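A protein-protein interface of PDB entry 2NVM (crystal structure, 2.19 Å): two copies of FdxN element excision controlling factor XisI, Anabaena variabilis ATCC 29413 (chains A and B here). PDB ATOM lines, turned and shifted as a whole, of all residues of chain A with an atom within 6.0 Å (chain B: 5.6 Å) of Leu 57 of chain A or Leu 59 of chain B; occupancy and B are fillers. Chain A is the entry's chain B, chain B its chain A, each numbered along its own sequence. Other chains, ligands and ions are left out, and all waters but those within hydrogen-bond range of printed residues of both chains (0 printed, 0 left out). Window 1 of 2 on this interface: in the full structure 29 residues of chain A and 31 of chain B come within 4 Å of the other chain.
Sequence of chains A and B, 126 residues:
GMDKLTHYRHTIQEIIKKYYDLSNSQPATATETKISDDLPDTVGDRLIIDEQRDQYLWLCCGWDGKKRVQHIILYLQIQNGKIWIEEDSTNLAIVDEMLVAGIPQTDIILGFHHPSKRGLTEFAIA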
ATOM      1  N   ILE A  16      11.031 -16.803  14.308  1.00  0.00           N
ATOM      2  CA  ILE A  16      12.104 -17.244  15.232  1.00  0.00           C
ATOM      3  C   ILE A  16      11.640 -18.434  16.115  1.00  0.00           C
ATOM      4  O   ILE A  16      12.353 -19.438  16.205  1.00  0.00           O
ATOM      5  CB  ILE A  16      12.762 -16.040  16.021  1.00  0.00           C
ATOM      6  CG1 ILE A  16      14.178 -16.417  16.502  1.00  0.00           C
ATOM      7  CG2 ILE A  16      11.860 -15.540  17.156  1.00  0.00           C
ATOM      8  CD1 ILE A  16      14.932 -15.304  17.247  1.00  0.00           C
ATOM      9  N   ARG A  46      18.666 -21.483  23.867  1.00  0.00           N
ATOM     10  CA  ARG A  46      17.965 -20.429  24.621  1.00  0.00           C
ATOM     11  C   ARG A  46      17.447 -19.391  23.619  1.00  0.00           C
ATOM     12  O   ARG A  46      18.147 -19.049  22.658  1.00  0.00           O
ATOM     13  CB  ARG A  46      18.857 -19.694  25.648  1.00  0.00           C
ATOM     14  CG  ARG A  46      19.452 -20.511  26.819  1.00  0.00           C
ATOM     15  CD  ARG A  46      20.761 -21.182  26.456  1.00  0.00           C
ATOM     16  NE  ARG A  46      21.335 -21.981  27.557  1.00  0.00           N
ATOM     17  CZ  ARG A  46      22.190 -21.560  28.503  1.00  0.00           C
ATOM     18  NH1 ARG A  46      22.620 -20.305  28.558  1.00  0.00           N
ATOM     19  NH2 ARG A  46      22.622 -22.418  29.428  1.00  0.00           N
ATOM     20  N   LEU A  47      16.240 -18.883  23.868  1.00  0.00           N
ATOM     21  CA  LEU A  47      15.570 -17.878  23.034  1.00  0.00           C
ATOM     22  C   LEU A  47      15.558 -16.582  23.844  1.00  0.00           C
ATOM     23  O   LEU A  47      15.241 -16.621  25.037  1.00  0.00           O
ATOM     24  CB  LEU A  47      14.148 -18.358  22.707  1.00  0.00           C
ATOM     25  CG  LEU A  47      13.397 -17.721  21.542  1.00  0.00           C
ATOM     26  CD1 LEU A  47      14.193 -17.862  20.249  1.00  0.00           C
ATOM     27  CD2 LEU A  47      11.995 -18.376  21.401  1.00  0.00           C
ATOM     28  N   ILE A  48      15.940 -15.460  23.215  1.00  0.00           N
ATOM     29  CA  ILE A  48      16.020 -14.152  23.896  1.00  0.00           C
ATOM     30  C   ILE A  48      15.300 -13.137  23.008  1.00  0.00           C
ATOM     31  O   ILE A  48      15.850 -12.654  22.000  1.00  0.00           O
ATOM     32  CB  ILE A  48      17.501 -13.719  24.216  1.00  0.00           C
ATOM     33  CG1 ILE A  48      18.355 -14.917  24.682  1.00  0.00           C
ATOM     34  CG2 ILE A  48      17.523 -12.537  25.233  1.00  0.00           C
ATOM     35  CD1 ILE A  48      19.764 -14.574  25.078  1.00  0.00           C
ATOM     36  N   ILE A  49      14.055 -12.850  23.373  1.00  0.00           N
ATOM     37  CA  ILE A  49      13.182 -11.926  22.652  1.00  0.00           C
ATOM     38  C   ILE A  49      13.045 -10.632  23.465  1.00  0.00           C
ATOM     39  O   ILE A  49      12.658 -10.678  24.611  1.00  0.00           O
ATOM     40  CB  ILE A  49      11.756 -12.543  22.449  1.00  0.00           C
ATOM     41  CG1 ILE A  49      11.819 -13.952  21.811  1.00  0.00           C
ATOM     42  CG2 ILE A  49      10.849 -11.594  21.659  1.00  0.00           C
ATOM     43  CD1 ILE A  49      12.502 -14.033  20.499  1.00  0.00           C
ATOM     44  N   GLN A  55      15.092  -6.774  19.406  1.00  0.00           N
ATOM     45  CA  GLN A  55      16.243  -7.687  19.333  1.00  0.00           C
ATOM     46  C   GLN A  55      15.663  -9.068  19.589  1.00  0.00           C
ATOM     47  O   GLN A  55      14.971  -9.274  20.602  1.00  0.00           O
ATOM     48  CB  GLN A  55      17.283  -7.327  20.384  1.00  0.00           C
ATOM     49  CG  GLN A  55      17.844  -5.901  20.285  1.00  0.00           C
ATOM     50  CD  GLN A  55      18.629  -5.644  19.023  1.00  0.00           C
ATOM     51  OE1 GLN A  55      19.441  -6.459  18.620  1.00  0.00           O
ATOM     52  NE2 GLN A  55      18.405  -4.493  18.403  1.00  0.00           N
ATOM     53  N   TYR A  56      15.925  -9.989  18.663  1.00  0.00           N
ATOM     54  CA  TYR A  56      15.384 -11.358  18.674  1.00  0.00           C
ATOM     55  C   TYR A  56      16.544 -12.303  18.410  1.00  0.00           C
ATOM     56  O   TYR A  56      17.089 -12.310  17.304  1.00  0.00           O
ATOM     57  CB  TYR A  56      14.287 -11.479  17.579  1.00  0.00           C
ATOM     58  CG  TYR A  56      13.243 -10.382  17.702  1.00  0.00           C
ATOM     59  CD1 TYR A  56      12.154 -10.507  18.579  1.00  0.00           C
ATOM     60  CD2 TYR A  56      13.380  -9.183  16.979  1.00  0.00           C
ATOM     61  CE1 TYR A  56      11.205  -9.460  18.721  1.00  0.00           C
ATOM     62  CE2 TYR A  56      12.433  -8.137  17.107  1.00  0.00           C
ATOM     63  CZ  TYR A  56      11.365  -8.272  17.981  1.00  0.00           C
ATOM     64  OH  TYR A  56      10.467  -7.241  18.092  1.00  0.00           O
ATOM     65  N   LEU A  57      16.908 -13.110  19.402  1.00  0.00           N
ATOM     66  CA  LEU A  57      18.056 -13.995  19.281  1.00  0.00           C
ATOM     67  C   LEU A  57      17.846 -15.402  19.825  1.00  0.00           C
ATOM     68  O   LEU A  57      17.184 -15.598  20.823  1.00  0.00           O
ATOM     69  CB  LEU A  57      19.243 -13.301  19.945  1.00  0.00           C
ATOM     70  CG  LEU A  57      20.622 -13.987  19.867  1.00  0.00           C
ATOM     71  CD1 LEU A  57      21.723 -13.001  19.485  1.00  0.00           C
ATOM     72  CD2 LEU A  57      20.927 -14.771  21.149  1.00  0.00           C
ATOM     73  N   TRP A  58      18.436 -16.357  19.121  1.00  0.00           N
ATOM     74  CA  TRP A  58      18.441 -17.756  19.433  1.00  0.00           C
ATOM     75  C   TRP A  58      19.907 -18.169  19.441  1.00  0.00           C
ATOM     76  O   TRP A  58      20.612 -18.012  18.428  1.00  0.00           O
ATOM     77  CB  TRP A  58      17.592 -18.523  18.390  1.00  0.00           C
ATOM     78  CG  TRP A  58      17.733 -20.011  18.354  1.00  0.00           C
ATOM     79  CD1 TRP A  58      18.103 -20.828  19.386  1.00  0.00           C
ATOM     80  CD2 TRP A  58      17.354 -20.881  17.275  1.00  0.00           C
ATOM     81  NE1 TRP A  58      18.058 -22.134  18.990  1.00  0.00           N
ATOM     82  CE2 TRP A  58      17.604 -22.211  17.707  1.00  0.00           C
ATOM     83  CE3 TRP A  58      16.861 -20.670  15.973  1.00  0.00           C
ATOM     84  CZ2 TRP A  58      17.380 -23.338  16.886  1.00  0.00           C
ATOM     85  CZ3 TRP A  58      16.629 -21.803  15.137  1.00  0.00           C
ATOM     86  CH2 TRP A  58      16.898 -23.121  15.606  1.00  0.00           C
ATOM     87  N   LEU A  59      20.350 -18.676  20.595  1.00  0.00           N
ATOM     88  CA  LEU A  59      21.700 -19.182  20.777  1.00  0.00           C
ATOM     89  C   LEU A  59      21.691 -20.511  21.493  1.00  0.00           C
ATOM     90  O   LEU A  59      20.667 -20.912  22.032  1.00  0.00           O
ATOM     91  CB  LEU A  59      22.546 -18.163  21.555  1.00  0.00           C
ATOM     92  CG  LEU A  59      22.195 -17.690  22.976  1.00  0.00           C
ATOM     93  CD1 LEU A  59      22.228 -18.766  24.023  1.00  0.00           C
ATOM     94  CD2 LEU A  59      23.210 -16.613  23.369  1.00  0.00           C
ATOM     95  N   ILE A  72      25.710 -18.208  18.521  1.00  0.00           N
ATOM     96  CA  ILE A  72      24.490 -17.561  17.977  1.00  0.00           C
ATOM     97  C   ILE A  72      24.042 -18.390  16.773  1.00  0.00           C
ATOM     98  O   ILE A  72      24.863 -18.654  15.887  1.00  0.00           O
ATOM     99  CB  ILE A  72      24.755 -16.085  17.603  1.00  0.00           C
ATOM    100  CG1 ILE A  72      25.121 -15.306  18.888  1.00  0.00           C
ATOM    101  CG2 ILE A  72      23.524 -15.453  16.848  1.00  0.00           C
ATOM    102  CD1 ILE A  72      25.475 -13.850  18.666  1.00  0.00           C
ATOM    103  N   LEU A  74      20.514 -17.864  15.335  1.00  0.00           N
ATOM    104  CA  LEU A  74      19.665 -16.953  14.575  1.00  0.00           C
ATOM    105  C   LEU A  74      19.540 -15.650  15.339  1.00  0.00           C
ATOM    106  O   LEU A  74      19.234 -15.670  16.540  1.00  0.00           O
ATOM    107  CB  LEU A  74      18.300 -17.626  14.364  1.00  0.00           C
ATOM    108  CG  LEU A  74      17.222 -17.113  13.398  1.00  0.00           C
ATOM    109  CD1 LEU A  74      17.759 -16.877  12.013  1.00  0.00           C
ATOM    110  CD2 LEU A  74      16.085 -18.143  13.331  1.00  0.00           C
ATOM    111  N   TYR A  75      19.810 -14.538  14.649  1.00  0.00           N
ATOM    112  CA  TYR A  75      19.762 -13.213  15.234  1.00  0.00           C
ATOM    113  C   TYR A  75      19.134 -12.234  14.241  1.00  0.00           C
ATOM    114  O   TYR A  75      19.633 -12.050  13.128  1.00  0.00           O
ATOM    115  CB  TYR A  75      21.171 -12.775  15.725  1.00  0.00           C
ATOM    116  CG  TYR A  75      21.281 -11.358  16.260  1.00  0.00           C
ATOM    117  CD1 TYR A  75      20.216 -10.742  16.974  1.00  0.00           C
ATOM    118  CD2 TYR A  75      22.494 -10.650  16.158  1.00  0.00           C
ATOM    119  CE1 TYR A  75      20.323  -9.434  17.468  1.00  0.00           C
ATOM    120  CE2 TYR A  75      22.617  -9.349  16.652  1.00  0.00           C
ATOM    121  CZ  TYR A  75      21.519  -8.751  17.321  1.00  0.00           C
ATOM    122  OH  TYR A  75      21.603  -7.485  17.833  1.00  0.00           O
ATOM    123  N   LEU A  76      18.040 -11.622  14.685  1.00  0.00           N
ATOM    124  CA  LEU A  76      17.265 -10.661  13.916  1.00  0.00           C
ATOM    125  C   LEU A  76      17.010  -9.417  14.752  1.00  0.00           C
ATOM    126  O   LEU A  76      16.811  -9.518  15.972  1.00  0.00           O
ATOM    127  CB  LEU A  76      15.909 -11.275  13.541  1.00  0.00           C
ATOM    128  CG  LEU A  76      15.893 -12.641  12.846  1.00  0.00           C
ATOM    129  CD1 LEU A  76      14.479 -13.106  12.622  1.00  0.00           C
ATOM    130  CD2 LEU A  76      16.593 -12.587  11.528  1.00  0.00           C
ATOM    131  N   GLY B  44      28.606  -1.985  16.678  1.00  0.00           N
ATOM    132  CA  GLY B  44      27.760  -1.323  17.680  1.00  0.00           C
ATOM    133  C   GLY B  44      27.222  -2.325  18.711  1.00  0.00           C
ATOM    134  O   GLY B  44      26.983  -3.489  18.398  1.00  0.00           O
ATOM    135  N   ASP B  45      27.001  -1.831  19.918  1.00  0.00           N
ATOM    136  CA  ASP B  45      26.508  -2.604  21.053  1.00  0.00           C
ATOM    137  C   ASP B  45      24.988  -2.704  21.013  1.00  0.00           C
ATOM    138  O   ASP B  45      24.322  -1.734  20.646  1.00  0.00           O
ATOM    139  CB  ASP B  45      26.872  -1.901  22.376  1.00  0.00           C
ATOM    140  CG  ASP B  45      28.376  -1.814  22.615  1.00  0.00           C
ATOM    141  OD1 ASP B  45      29.057  -2.855  22.579  1.00  0.00           O
ATOM    142  OD2 ASP B  45      28.860  -0.707  22.931  1.00  0.00           O
ATOM    143  N   ARG B  46      24.474  -3.876  21.385  1.00  0.00           N
ATOM    144  CA  ARG B  46      23.031  -4.150  21.459  1.00  0.00           C
ATOM    145  C   ARG B  46      22.753  -4.852  22.785  1.00  0.00           C
ATOM    146  O   ARG B  46      23.528  -5.710  23.200  1.00  0.00           O
ATOM    147  CB  ARG B  46      22.494  -5.037  20.315  1.00  0.00           C
ATOM    148  CG  ARG B  46      22.631  -4.493  18.880  1.00  0.00           C
ATOM    149  CD  ARG B  46      23.957  -4.840  18.236  1.00  0.00           C
ATOM    150  NE  ARG B  46      24.119  -4.198  16.920  1.00  0.00           N
ATOM    151  CZ  ARG B  46      23.630  -4.634  15.750  1.00  0.00           C
ATOM    152  NH1 ARG B  46      22.901  -5.745  15.664  1.00  0.00           N
ATOM    153  NH2 ARG B  46      23.875  -3.946  14.641  1.00  0.00           N
ATOM    154  N   LEU B  47      21.655  -4.464  23.433  1.00  0.00           N
ATOM    155  CA  LEU B  47      21.183  -5.025  24.674  1.00  0.00           C
ATOM    156  C   LEU B  47      19.916  -5.820  24.317  1.00  0.00           C
ATOM    157  O   LEU B  47      19.066  -5.325  23.570  1.00  0.00           O
ATOM    158  CB  LEU B  47      20.888  -3.885  25.662  1.00  0.00           C
ATOM    159  CG  LEU B  47      20.729  -4.223  27.143  1.00  0.00           C
ATOM    160  CD1 LEU B  47      21.991  -4.897  27.668  1.00  0.00           C
ATOM    161  CD2 LEU B  47      20.385  -2.952  27.953  1.00  0.00           C
ATOM    162  N   ILE B  48      19.830  -7.062  24.791  1.00  0.00           N
ATOM    163  CA  ILE B  48      18.689  -7.951  24.540  1.00  0.00           C
ATOM    164  C   ILE B  48      18.242  -8.508  25.912  1.00  0.00           C
ATOM    165  O   ILE B  48      18.897  -9.400  26.478  1.00  0.00           O
ATOM    166  CB  ILE B  48      19.033  -9.096  23.564  1.00  0.00           C
ATOM    167  CG1 ILE B  48      19.941  -8.622  22.414  1.00  0.00           C
ATOM    168  CG2 ILE B  48      17.728  -9.771  23.064  1.00  0.00           C
ATOM    169  CD1 ILE B  48      20.173  -9.701  21.315  1.00  0.00           C
ATOM    170  N   LEU B  57      21.320 -10.253  27.836  1.00  0.00           N
ATOM    171  CA  LEU B  57      22.515 -10.314  26.997  1.00  0.00           C
ATOM    172  C   LEU B  57      22.886  -9.010  26.343  1.00  0.00           C
ATOM    173  O   LEU B  57      22.021  -8.234  25.904  1.00  0.00           O
ATOM    174  CB  LEU B  57      22.347 -11.421  25.936  1.00  0.00           C
ATOM    175  CG  LEU B  57      23.465 -11.781  24.915  1.00  0.00           C
ATOM    176  CD1 LEU B  57      23.369 -13.220  24.486  1.00  0.00           C
ATOM    177  CD2 LEU B  57      23.438 -10.906  23.685  1.00  0.00           C
ATOM    178  N   TRP B  58      24.197  -8.792  26.313  1.00  0.00           N
ATOM    179  CA  TRP B  58      24.823  -7.644  25.701  1.00  0.00           C
ATOM    180  C   TRP B  58      25.857  -8.196  24.729  1.00  0.00           C
ATOM    181  O   TRP B  58      26.734  -8.958  25.126  1.00  0.00           O
ATOM    182  CB  TRP B  58      25.409  -6.719  26.773  1.00  0.00           C
ATOM    183  CG  TRP B  58      26.413  -5.700  26.298  1.00  0.00           C
ATOM    184  CD1 TRP B  58      26.476  -5.099  25.078  1.00  0.00           C
ATOM    185  CD2 TRP B  58      27.426  -5.088  27.096  1.00  0.00           C
ATOM    186  NE1 TRP B  58      27.520  -4.233  25.039  1.00  0.00           N
ATOM    187  CE2 TRP B  58      28.111  -4.172  26.265  1.00  0.00           C
ATOM    188  CE3 TRP B  58      27.835  -5.234  28.431  1.00  0.00           C
ATOM    189  CZ2 TRP B  58      29.198  -3.408  26.712  1.00  0.00           C
ATOM    190  CZ3 TRP B  58      28.939  -4.488  28.881  1.00  0.00           C
ATOM    191  CH2 TRP B  58      29.599  -3.577  28.020  1.00  0.00           C
ATOM    192  N   LEU B  59      25.681  -7.846  23.454  1.00  0.00           N
ATOM    193  CA  LEU B  59      26.596  -8.226  22.386  1.00  0.00           C
ATOM    194  C   LEU B  59      26.959  -7.012  21.550  1.00  0.00           C
ATOM    195  O   LEU B  59      26.375  -5.929  21.716  1.00  0.00           O
ATOM    196  CB  LEU B  59      25.992  -9.340  21.521  1.00  0.00           C
ATOM    197  CG  LEU B  59      24.655  -9.161  20.765  1.00  0.00           C
ATOM    198  CD1 LEU B  59      24.691  -8.075  19.701  1.00  0.00           C
ATOM    199  CD2 LEU B  59      24.272 -10.458  20.078  1.00  0.00           C
ATOM    200  N   CYS B  60      27.985  -7.171  20.720  1.00  0.00           N
ATOM    201  CA  CYS B  60      28.354  -6.149  19.755  1.00  0.00           C
ATOM    202  C   CYS B  60      28.298  -6.841  18.377  1.00  0.00           C
ATOM    203  O   CYS B  60      28.567  -8.051  18.243  1.00  0.00           O
ATOM    204  CB  CYS B  60      29.674  -5.442  20.066  1.00  0.00           C
ATOM    205  SG  CYS B  60      31.072  -6.446  19.903  1.00  0.00           S
ATOM    206  N   CYS B  61      27.909  -6.074  17.364  1.00  0.00           N
ATOM    207  CA  CYS B  61      27.717  -6.617  16.027  1.00  0.00           C
ATOM    208  C   CYS B  61      27.950  -5.562  14.960  1.00  0.00           C
ATOM    209  O   CYS B  61      27.554  -4.407  15.131  1.00  0.00           O
ATOM    210  CB  CYS B  61      26.315  -7.200  15.956  1.00  0.00           C
ATOM    211  SG  CYS B  61      25.806  -7.921  14.407  1.00  0.00           S
ATOM    212  N   GLN B  70      30.729 -10.237  15.709  1.00  0.00           N
ATOM    213  CA  GLN B  70      29.465 -10.699  16.330  1.00  0.00           C
ATOM    214  C   GLN B  70      29.915 -11.407  17.606  1.00  0.00           C
ATOM    215  O   GLN B  70      30.218 -12.596  17.585  1.00  0.00           O
ATOM    216  CB  GLN B  70      28.661 -11.587  15.374  1.00  0.00           C
ATOM    217  CG  GLN B  70      27.266 -11.882  15.874  1.00  0.00           C
ATOM    218  CD  GLN B  70      26.491 -12.701  14.883  1.00  0.00           C
ATOM    219  OE1 GLN B  70      25.645 -12.165  14.165  1.00  0.00           O
ATOM    220  NE2 GLN B  70      26.825 -13.991  14.775  1.00  0.00           N
ATOM    221  N   HIS B  71      29.966 -10.641  18.690  1.00  0.00           N
ATOM    222  CA  HIS B  71      30.577 -11.049  19.941  1.00  0.00           C
ATOM    223  C   HIS B  71      29.724 -10.750  21.189  1.00  0.00           C
ATOM    224  O   HIS B  71      29.337  -9.614  21.412  1.00  0.00           O
ATOM    225  CB  HIS B  71      31.947 -10.301  19.969  1.00  0.00           C
ATOM    226  CG  HIS B  71      32.690 -10.386  21.260  1.00  0.00           C
ATOM    227  ND1 HIS B  71      33.356 -11.522  21.662  1.00  0.00           N
ATOM    228  CD2 HIS B  71      32.904  -9.462  22.223  1.00  0.00           C
ATOM    229  CE1 HIS B  71      33.924 -11.305  22.836  1.00  0.00           C
ATOM    230  NE2 HIS B  71      33.663 -10.061  23.200  1.00  0.00           N
ATOM    231  N   ILE B  72      29.482 -11.792  21.992  1.00  0.00           N
ATOM    232  CA  ILE B  72      28.747 -11.715  23.261  1.00  0.00           C
ATOM    233  C   ILE B  72      29.724 -11.142  24.298  1.00  0.00           C
ATOM    234  O   ILE B  72      30.815 -11.672  24.503  1.00  0.00           O
ATOM    235  CB  ILE B  72      28.206 -13.118  23.692  1.00  0.00           C
ATOM    236  CG1 ILE B  72      27.195 -13.620  22.654  1.00  0.00           C
ATOM    237  CG2 ILE B  72      27.601 -13.085  25.110  1.00  0.00           C
ATOM    238  CD1 ILE B  72      26.754 -15.081  22.861  1.00  0.00           C
ATOM    239  N   ILE B  73      29.326 -10.038  24.921  1.00  0.00           N
ATOM    240  CA  ILE B  73      30.128  -9.326  25.918  1.00  0.00           C
ATOM    241  C   ILE B  73      29.729  -9.742  27.343  1.00  0.00           C
ATOM    242  O   ILE B  73      30.597 -10.051  28.171  1.00  0.00           O
ATOM    243  CB  ILE B  73      29.987  -7.795  25.732  1.00  0.00           C
ATOM    244  CG1 ILE B  73      30.446  -7.393  24.298  1.00  0.00           C
ATOM    245  CG2 ILE B  73      30.791  -7.029  26.852  1.00  0.00           C
ATOM    246  CD1 ILE B  73      30.226  -5.917  23.933  1.00  0.00           C
ATOM    247  N   LEU B  74      28.426  -9.744  27.611  1.00  0.00           N
ATOM    248  CA  LEU B  74      27.901 -10.062  28.931  1.00  0.00           C
ATOM    249  C   LEU B  74      26.607 -10.856  28.750  1.00  0.00           C
ATOM    250  O   LEU B  74      25.755 -10.485  27.912  1.00  0.00           O
ATOM    251  CB  LEU B  74      27.760  -8.708  29.691  1.00  0.00           C
ATOM    252  CG  LEU B  74      27.699  -8.590  31.203  1.00  0.00           C
ATOM    253  CD1 LEU B  74      28.872  -9.246  31.850  1.00  0.00           C
ATOM    254  CD2 LEU B  74      27.629  -7.125  31.664  1.00  0.00           C
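Ile 48 of chain B touches Ile 48 of chain A. Leu 57 of chain B touches Ile 48 of chain A. CG of Arg 46 of chain B touches OE1 of Gln 55 of chain A, at 3.8 Å. CG of Gln 55 of chain A touches O of Leu 47 of chain B, 3.6 Å away. CB of Leu 57 of chain A touches CD1 of Ile 48 of chain B, 3.96 Å away. Leu 59 of chain B touches Leu 57 of chain A. CD2 of Leu 59 of chain A touches CD1 of Leu 57 of chain B, 3.6 Å away. Ile 72 of chain B touches Leu 59 of chain A. Gln 70 of chain B touches Ile 72 of chain A. Tyr 75 of chain A touches Ile 48 of chain B (CE1 to CD1, 3.9 Å).
Leu 59 of chain B touches just these residues of chain A: Leu 57 (3.6 Å), Ile 72 (3.9 Å) and Tyr 75 (3.7 Å). Of the printed residues of chain B, Ile 72 of chain A touches Leu 59 (3.9 Å) and Gln 70 (3.9 Å). Printed residues of chain B within 4 Å of Leu 59 of chain A: Leu 57 (3.6 Å) and Ile 72 (3.9 Å). Printed residues of chain A within 4 Å of Gln 70 of chain B: Ile 72 (3.9 Å). Leu 47 of chain A touches none of the printed residues of chain B. The nearest residue of chain A that does not touch Leu 59 of chain B is Gln 55 of chain A (5.6 Å).
NH1 of Arg 46 of chain B lies within hydrogen-bond range of OH of Tyr 75 of chain A, at 3.1 Å.
Hydrophobic or aromatic side chains of chain A within 4 Å of the printed part of chain B: Ile 48, Leu 57, Leu 59, Ile 72 and Tyr 75. Of the 15 printed residues of chain B, 7 touch a printed residue of chain A. Hydrophobic or aromatic side chains of chain B that line the printed part of chain A: Ile 48, Leu 57, Leu 59 and Ile 72. Among the printed residues, no Asp or Glu carboxylate lies within 4 Å of a Lys or Arg side-chain nitrogen of the other chain.
Ile 48 of chain A touches its own counterpart, Ile 48 of chain B. Ile 48 of chain A touches Leu 57 of chain B, and with the chains exchanged Leu 57 of chain A touches Ile 48 of chain B. Leu 57 of chain A touches Leu 59 of chain B, and with the chains exchanged Leu 59 of chain A touches Leu 57 of chain B. Leu 59 of chain A touches Ile 72 of chain B, and with the chains exchanged Ile 72 of chain A touches Leu 59 of chain B. Positions printed for both chains: 46, 47, 48, 57, 58, 59, 72 and 74.
NE of Arg 46 of chain B sits at hydrogen-bond distance from O of Gly 44 of chain B. N of Arg 46 of chain B sits at hydrogen-bond distance from O of Leu 59 of chain B (2.8 Å). The side-chain amide oxygen of Gln 55 of chain A sits at hydrogen-bond distance from the side-chain hydroxyl of Tyr 75 of chain A, at 2.5 Å. The backbone NH (N) of Ile 48 of chain B sits at hydrogen-bond distance from the backbone carbonyl oxygen (O) of Leu 57 of chain B, at 2.7 Å. N of Ile 48 of chain A is in hydrogen-bond range of O of Leu 57 of chain A (2.7 Å). N of Arg 46 of chain A is in hydrogen-bond range of O of Leu 59 of chain A.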
